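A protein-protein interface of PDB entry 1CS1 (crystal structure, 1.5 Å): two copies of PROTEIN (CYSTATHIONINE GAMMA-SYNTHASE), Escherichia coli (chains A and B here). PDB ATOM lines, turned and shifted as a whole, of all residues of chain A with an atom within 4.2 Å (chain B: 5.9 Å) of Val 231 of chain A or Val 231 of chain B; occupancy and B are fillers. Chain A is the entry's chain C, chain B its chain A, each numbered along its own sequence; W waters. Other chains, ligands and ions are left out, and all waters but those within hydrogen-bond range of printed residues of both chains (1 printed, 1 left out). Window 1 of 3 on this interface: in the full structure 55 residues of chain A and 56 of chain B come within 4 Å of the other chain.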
ATOM      1  N   THR A  73      -9.438  32.845   7.844  1.00  0.00           N
ATOM      2  CA  THR A  73     -10.286  32.398   6.751  1.00  0.00           C
ATOM      3  C   THR A  73      -9.648  31.179   6.063  1.00  0.00           C
ATOM      4  O   THR A  73      -8.491  30.850   6.327  1.00  0.00           O
ATOM      5  CB  THR A  73     -10.513  33.553   5.757  1.00  0.00           C
ATOM      6  OG1 THR A  73      -9.258  33.979   5.212  1.00  0.00           O
ATOM      7  CG2 THR A  73     -11.152  34.737   6.476  1.00  0.00           C
ATOM      8  N   ASN A  74     -10.381  30.522   5.170  1.00  0.00           N
ATOM      9  CA  ASN A  74      -9.850  29.319   4.531  1.00  0.00           C
ATOM     10  C   ASN A  74      -8.801  29.513   3.443  1.00  0.00           C
ATOM     11  O   ASN A  74      -8.091  28.573   3.097  1.00  0.00           O
ATOM     12  CB  ASN A  74     -10.993  28.451   4.013  1.00  0.00           C
ATOM     13  CG  ASN A  74     -11.706  29.074   2.863  1.00  0.00           C
ATOM     14  OD1 ASN A  74     -12.323  30.126   3.003  1.00  0.00           O
ATOM     15  ND2 ASN A  74     -11.622  28.436   1.703  1.00  0.00           N
ATOM     16  N   SER A  78     -10.082  34.464   0.288  1.00  0.00           N
ATOM     17  CA  SER A  78     -11.342  34.643   0.989  1.00  0.00           C
ATOM     18  C   SER A  78     -11.199  35.654   2.124  1.00  0.00           C
ATOM     19  O   SER A  78     -12.198  36.168   2.635  1.00  0.00           O
ATOM     20  CB  SER A  78     -11.920  33.298   1.465  1.00  0.00           C
ATOM     21  OG  SER A  78     -11.194  32.723   2.529  1.00  0.00           O
ATOM     22  N   ALA A 226     -17.837  36.339   8.415  1.00  0.00           N
ATOM     23  CA  ALA A 226     -17.103  35.142   7.974  1.00  0.00           C
ATOM     24  C   ALA A 226     -17.946  33.896   8.224  1.00  0.00           C
ATOM     25  O   ALA A 226     -17.926  32.946   7.439  1.00  0.00           O
ATOM     26  CB  ALA A 226     -15.758  35.029   8.693  1.00  0.00           C
ATOM     27  N   ILE A 229     -21.104  34.039   5.435  1.00  0.00           N
ATOM     28  CA  ILE A 229     -20.822  33.618   4.069  1.00  0.00           C
ATOM     29  C   ILE A 229     -20.008  32.322   4.017  1.00  0.00           C
ATOM     30  O   ILE A 229     -19.726  31.785   2.945  1.00  0.00           O
ATOM     31  CB  ILE A 229     -20.145  34.763   3.271  1.00  0.00           C
ATOM     32  CG1 ILE A 229     -18.726  35.052   3.784  1.00  0.00           C
ATOM     33  CG2 ILE A 229     -21.023  36.008   3.368  1.00  0.00           C
ATOM     34  CD1 ILE A 229     -17.906  35.970   2.834  1.00  0.00           C
ATOM     35  N   GLY A 230     -19.641  31.831   5.190  1.00  0.00           N
ATOM     36  CA  GLY A 230     -18.942  30.566   5.294  1.00  0.00           C
ATOM     37  C   GLY A 230     -17.462  30.480   5.010  1.00  0.00           C
ATOM     38  O   GLY A 230     -17.006  29.420   4.589  1.00  0.00           O
ATOM     39  N   VAL A 231     -16.691  31.533   5.276  1.00  0.00           N
ATOM     40  CA  VAL A 231     -15.262  31.474   4.962  1.00  0.00           C
ATOM     41  C   VAL A 231     -14.257  31.268   6.096  1.00  0.00           C
ATOM     42  O   VAL A 231     -13.068  31.507   5.908  1.00  0.00           O
ATOM     43  CB  VAL A 231     -14.817  32.728   4.131  1.00  0.00           C
ATOM     44  CG1 VAL A 231     -15.514  32.715   2.763  1.00  0.00           C
ATOM     45  CG2 VAL A 231     -15.127  34.026   4.895  1.00  0.00           C
ATOM     46  N   THR A 232     -14.710  30.821   7.262  1.00  0.00           N
ATOM     47  CA  THR A 232     -13.792  30.586   8.376  1.00  0.00           C
ATOM     48  C   THR A 232     -12.872  29.414   8.033  1.00  0.00           C
ATOM     49  O   THR A 232     -13.296  28.444   7.402  1.00  0.00           O
ATOM     50  CB  THR A 232     -14.559  30.254   9.653  1.00  0.00           C
ATOM     51  OG1 THR A 232     -15.560  29.267   9.372  1.00  0.00           O
ATOM     52  CG2 THR A 232     -15.236  31.494  10.186  1.00  0.00           C
ATOM     53  N   GLY A 233     -11.613  29.494   8.453  1.00  0.00           N
ATOM     54  CA  GLY A 233     -10.668  28.434   8.143  1.00  0.00           C
ATOM     55  C   GLY A 233     -10.849  27.166   8.950  1.00  0.00           C
ATOM     56  O   GLY A 233     -11.474  27.186  10.007  1.00  0.00           O
ATOM     57  N   LEU B  72     -15.862  21.083  -4.325  1.00  0.00           N
ATOM     58  CA  LEU B  72     -15.862  21.018  -2.868  1.00  0.00           C
ATOM     59  C   LEU B  72     -15.482  22.372  -2.269  1.00  0.00           C
ATOM     60  O   LEU B  72     -14.418  22.920  -2.585  1.00  0.00           O
ATOM     61  CB  LEU B  72     -14.883  19.940  -2.360  1.00  0.00           C
ATOM     62  CG  LEU B  72     -14.968  19.706  -0.832  1.00  0.00           C
ATOM     63  CD1 LEU B  72     -16.051  18.691  -0.563  1.00  0.00           C
ATOM     64  CD2 LEU B  72     -13.646  19.216  -0.249  1.00  0.00           C
ATOM     65  N   THR B  73     -16.346  22.905  -1.403  1.00  0.00           N
ATOM     66  CA  THR B  73     -16.100  24.182  -0.747  1.00  0.00           C
ATOM     67  C   THR B  73     -15.740  23.980   0.732  1.00  0.00           C
ATOM     68  O   THR B  73     -15.904  22.891   1.280  1.00  0.00           O
ATOM     69  CB  THR B  73     -17.324  25.126  -0.888  1.00  0.00           C
ATOM     70  OG1 THR B  73     -18.435  24.602  -0.148  1.00  0.00           O
ATOM     71  CG2 THR B  73     -17.717  25.263  -2.357  1.00  0.00           C
ATOM     72  N   ASN B  74     -15.260  25.025   1.394  1.00  0.00           N
ATOM     73  CA  ASN B  74     -14.841  24.853   2.774  1.00  0.00           C
ATOM     74  C   ASN B  74     -15.938  24.673   3.813  1.00  0.00           C
ATOM     75  O   ASN B  74     -15.656  24.206   4.903  1.00  0.00           O
ATOM     76  CB  ASN B  74     -13.855  25.959   3.181  1.00  0.00           C
ATOM     77  CG  ASN B  74     -14.496  27.304   3.282  1.00  0.00           C
ATOM     78  OD1 ASN B  74     -14.979  27.853   2.284  1.00  0.00           O
ATOM     79  ND2 ASN B  74     -14.501  27.865   4.490  1.00  0.00           N
ATOM     80  N   THR B  75     -17.172  25.055   3.489  1.00  0.00           N
ATOM     81  CA  THR B  75     -18.323  24.850   4.376  1.00  0.00           C
ATOM     82  C   THR B  75     -19.571  24.743   3.502  1.00  0.00           C
ATOM     83  O   THR B  75     -19.540  25.094   2.326  1.00  0.00           O
ATOM     84  CB  THR B  75     -18.578  26.015   5.391  1.00  0.00           C
ATOM     85  OG1 THR B  75     -18.898  27.218   4.680  1.00  0.00           O
ATOM     86  CG2 THR B  75     -17.380  26.241   6.288  1.00  0.00           C
ATOM     87  N   SER B  78     -20.577  28.151   2.433  1.00  0.00           N
ATOM     88  CA  SER B  78     -19.822  28.757   1.339  1.00  0.00           C
ATOM     89  C   SER B  78     -20.193  28.132  -0.005  1.00  0.00           C
ATOM     90  O   SER B  78     -19.947  28.726  -1.049  1.00  0.00           O
ATOM     91  CB  SER B  78     -18.297  28.719   1.596  1.00  0.00           C
ATOM     92  OG  SER B  78     -17.710  27.448   1.383  1.00  0.00           O
ATOM     93  N   HIS B  81     -23.144  30.227  -0.800  1.00  0.00           N
ATOM     94  CA  HIS B  81     -22.652  31.558  -1.175  1.00  0.00           C
ATOM     95  C   HIS B  81     -22.018  31.511  -2.559  1.00  0.00           C
ATOM     96  O   HIS B  81     -22.120  32.465  -3.316  1.00  0.00           O
ATOM     97  CB  HIS B  81     -21.620  32.045  -0.158  1.00  0.00           C
ATOM     98  CG  HIS B  81     -21.093  33.426  -0.428  1.00  0.00           C
ATOM     99  ND1 HIS B  81     -21.909  34.535  -0.527  1.00  0.00           N
ATOM    100  CD2 HIS B  81     -19.824  33.885  -0.545  1.00  0.00           C
ATOM    101  CE1 HIS B  81     -21.167  35.615  -0.688  1.00  0.00           C
ATOM    102  NE2 HIS B  81     -19.898  35.249  -0.703  1.00  0.00           N
ATOM    103  N   LEU B  82     -21.369  30.390  -2.880  1.00  0.00           N
ATOM    104  CA  LEU B  82     -20.735  30.206  -4.187  1.00  0.00           C
ATOM    105  C   LEU B  82     -21.787  30.215  -5.282  1.00  0.00           C
ATOM    106  O   LEU B  82     -21.649  30.919  -6.280  1.00  0.00           O
ATOM    107  CB  LEU B  82     -19.981  28.868  -4.257  1.00  0.00           C
ATOM    108  CG  LEU B  82     -19.406  28.499  -5.643  1.00  0.00           C
ATOM    109  CD1 LEU B  82     -18.378  29.528  -6.088  1.00  0.00           C
ATOM    110  CD2 LEU B  82     -18.764  27.123  -5.589  1.00  0.00           C
ATOM    111  N   TRP B 225     -15.239  30.310 -10.212  1.00  0.00           N
ATOM    112  CA  TRP B 225     -15.648  31.238  -9.164  1.00  0.00           C
ATOM    113  C   TRP B 225     -15.196  30.836  -7.762  1.00  0.00           C
ATOM    114  O   TRP B 225     -14.914  31.701  -6.939  1.00  0.00           O
ATOM    115  CB  TRP B 225     -17.162  31.423  -9.197  1.00  0.00           C
ATOM    116  CG  TRP B 225     -17.551  32.395 -10.249  1.00  0.00           C
ATOM    117  CD1 TRP B 225     -17.926  32.117 -11.535  1.00  0.00           C
ATOM    118  CD2 TRP B 225     -17.524  33.819 -10.134  1.00  0.00           C
ATOM    119  NE1 TRP B 225     -18.129  33.289 -12.226  1.00  0.00           N
ATOM    120  CE2 TRP B 225     -17.889  34.348 -11.390  1.00  0.00           C
ATOM    121  CE3 TRP B 225     -17.221  34.701  -9.089  1.00  0.00           C
ATOM    122  CZ2 TRP B 225     -17.962  35.718 -11.629  1.00  0.00           C
ATOM    123  CZ3 TRP B 225     -17.290  36.065  -9.327  1.00  0.00           C
ATOM    124  CH2 TRP B 225     -17.659  36.558 -10.587  1.00  0.00           C
ATOM    125  N   ALA B 226     -15.127  29.533  -7.487  1.00  0.00           N
ATOM    126  CA  ALA B 226     -14.708  29.062  -6.164  1.00  0.00           C
ATOM    127  C   ALA B 226     -13.274  29.509  -5.908  1.00  0.00           C
ATOM    128  O   ALA B 226     -12.921  29.906  -4.796  1.00  0.00           O
ATOM    129  CB  ALA B 226     -14.820  27.534  -6.077  1.00  0.00           C
ATOM    130  N   ASN B 227     -12.457  29.448  -6.953  1.00  0.00           N
ATOM    131  CA  ASN B 227     -11.072  29.865  -6.855  1.00  0.00           C
ATOM    132  C   ASN B 227     -11.012  31.388  -6.753  1.00  0.00           C
ATOM    133  O   ASN B 227     -10.268  31.940  -5.944  1.00  0.00           O
ATOM    134  CB  ASN B 227     -10.295  29.404  -8.086  1.00  0.00           C
ATOM    135  CG  ASN B 227      -8.871  29.917  -8.091  1.00  0.00           C
ATOM    136  OD1 ASN B 227      -8.104  29.664  -7.162  1.00  0.00           O
ATOM    137  ND2 ASN B 227      -8.512  30.654  -9.136  1.00  0.00           N
ATOM    138  N   ILE B 229     -13.170  33.649  -5.549  1.00  0.00           N
ATOM    139  CA  ILE B 229     -13.510  34.213  -4.241  1.00  0.00           C
ATOM    140  C   ILE B 229     -12.860  33.457  -3.074  1.00  0.00           C
ATOM    141  O   ILE B 229     -13.037  33.826  -1.916  1.00  0.00           O
ATOM    142  CB  ILE B 229     -15.066  34.292  -4.025  1.00  0.00           C
ATOM    143  CG1 ILE B 229     -15.685  32.893  -3.974  1.00  0.00           C
ATOM    144  CG2 ILE B 229     -15.707  35.113  -5.144  1.00  0.00           C
ATOM    145  CD1 ILE B 229     -17.179  32.882  -3.628  1.00  0.00           C
ATOM    146  N   GLY B 230     -12.113  32.400  -3.393  1.00  0.00           N
ATOM    147  CA  GLY B 230     -11.402  31.620  -2.380  1.00  0.00           C
ATOM    148  C   GLY B 230     -12.151  30.684  -1.439  1.00  0.00           C
ATOM    149  O   GLY B 230     -11.768  30.553  -0.275  1.00  0.00           O
ATOM    150  N   VAL B 231     -13.190  30.009  -1.923  1.00  0.00           N
ATOM    151  CA  VAL B 231     -13.962  29.107  -1.078  1.00  0.00           C
ATOM    152  C   VAL B 231     -13.736  27.607  -1.283  1.00  0.00           C
ATOM    153  O   VAL B 231     -14.518  26.796  -0.798  1.00  0.00           O
ATOM    154  CB  VAL B 231     -15.466  29.371  -1.221  1.00  0.00           C
ATOM    155  CG1 VAL B 231     -15.787  30.746  -0.680  1.00  0.00           C
ATOM    156  CG2 VAL B 231     -15.891  29.222  -2.685  1.00  0.00           C
ATOM    157  N   THR B 232     -12.678  27.225  -1.988  1.00  0.00           N
ATOM    158  CA  THR B 232     -12.414  25.805  -2.209  1.00  0.00           C
ATOM    159  C   THR B 232     -12.087  25.135  -0.864  1.00  0.00           C
ATOM    160  O   THR B 232     -11.530  25.773   0.040  1.00  0.00           O
ATOM    161  CB  THR B 232     -11.230  25.599  -3.198  1.00  0.00           C
ATOM    162  OG1 THR B 232     -10.151  26.484  -2.856  1.00  0.00           O
ATOM    163  CG2 THR B 232     -11.661  25.887  -4.631  1.00  0.00           C
ATOM    164  N   GLY B 233     -12.441  23.857  -0.730  1.00  0.00           N
ATOM    165  CA  GLY B 233     -12.182  23.132   0.505  1.00  0.00           C
ATOM    166  C   GLY B 233     -10.759  22.618   0.667  1.00  0.00           C
ATOM    167  O   GLY B 233     -10.056  22.365  -0.320  1.00  0.00           O
HETATM  168  O   HOH W   1     -12.851  26.445   5.872  1.00  0.00           O
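The side-chain amide nitrogen of Asn 74 of chain A lies within hydrogen-bond range of the side-chain amide oxygen of Asn 74 of chain B, 3.5 Å away. The backbone carbonyl oxygen of Gly 230 of chain A lies within hydrogen-bond range of the side-chain amide nitrogen of Asn 74 of chain B (3.0 Å). ND2 of Asn 74 of chain B sits at hydrogen-bond distance from O of Thr 232 of chain A, 3.2 Å away. The backbone carbonyl oxygen of Gly 230 of chain A lies within hydrogen-bond range of the side-chain hydroxyl of Thr 75 of chain B (2.9 Å). ND2 of Asn 74 of chain A lies within hydrogen-bond range of O of Gly 230 of chain B (2.9 Å). O of Thr 232 of chain B lies within hydrogen-bond range of ND2 of Asn 74 of chain A.
OG1 of Thr 73 of chain B sits at hydrogen-bond distance from O of Thr 75 of chain B, 2.8 Å away. The side-chain hydroxyl (OG) of Ser 78 of chain B sits at hydrogen-bond distance from the side-chain amide oxygen (OD1) of Asn 74 of chain B (2.9 Å). The backbone NH of Ser 78 of chain B is in hydrogen-bond range of the side-chain hydroxyl of Thr 75 of chain B (3.0 Å). The backbone carbonyl oxygen (O) of Ala 226 of chain B lies within hydrogen-bond range of the backbone NH (N) of Val 231 of chain B, at 2.9 Å. OD1 of Asn 74 of chain A lies within hydrogen-bond range of OG of Ser 78 of chain A, at 2.9 Å. The backbone NH (N) of Asn 74 of chain A sits at hydrogen-bond distance from the backbone carbonyl oxygen (O) of Val 231 of chain A, at 3.0 Å.
Among the printed residues, pairs that only touch across the chains: Asn 74 of chain A with Val 231 of chain B (3.7 Å), Ser 78 of chain A with Ile 229 of chain B (3.5 Å), Ser 78 of chain A with Gly 230 of chain B (3.3 Å), Ile 229 of chain A with Ser 78 of chain B (3.4 Å), Ile 229 of chain A with His 81 of chain B (3.6 Å), Gly 230 of chain A with Ser 78 of chain B (3.3 Å), Val 231 of chain A with Asn 74 of chain B (3.7 Å) and Val 231 of chain A with Val 231 of chain B (3.98 Å).
Of the printed residues of chain B, Asn 74 of chain A touches Asn 74 (3.3 Å), Gly 230 (2.9 Å), Val 231 (3.7 Å) and Thr 232 (3.1 Å). Thr 73 of chain B touches none of the printed residues of chain A. Printed residues of chain A within 4 Å of Thr 75 of chain B: Gly 230 (2.9 Å). Asn 227 of chain B touches none of the printed residues of chain A. The nearest printed residue of chain B that does not touch Asn 74 of chain A is Gly 233 of chain B (5.2 Å).
Of the 9 printed residues of chain A, 6 touch a printed residue of chain B. Among the printed residues, 14 pairs touch across the chains. Among the printed residues, no Asp or Glu carboxylate lies within 4 Å of a Lys or Arg side-chain nitrogen of the other chain.
Asn 74 of chain A touches Gly 230 of chain B, and with the chains exchanged Gly 230 of chain A touches Asn 74 of chain B. Asn 74 of chain A touches Val 231 of chain B, and with the chains exchanged Val 231 of chain A touches Asn 74 of chain B. Asn 74 of chain A touches Thr 232 of chain B, and with the chains exchanged Thr 232 of chain A touches Asn 74 of chain B. Ser 78 of chain A touches Ile 229 of chain B, and with the chains exchanged Ile 229 of chain A touches Ser 78 of chain B. Positions printed for both chains: 73, 74, 78, 226, 229, 230, 231, 232 and 233. Of the 14 pairs that touch across the chains among the printed residues, 12 have their exchanged pair printed and touching as well.
Water W1 bridges O of Thr 232 of chain A (2.6 Å) and ND2 of Asn 74 of chain B (2.6 Å).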
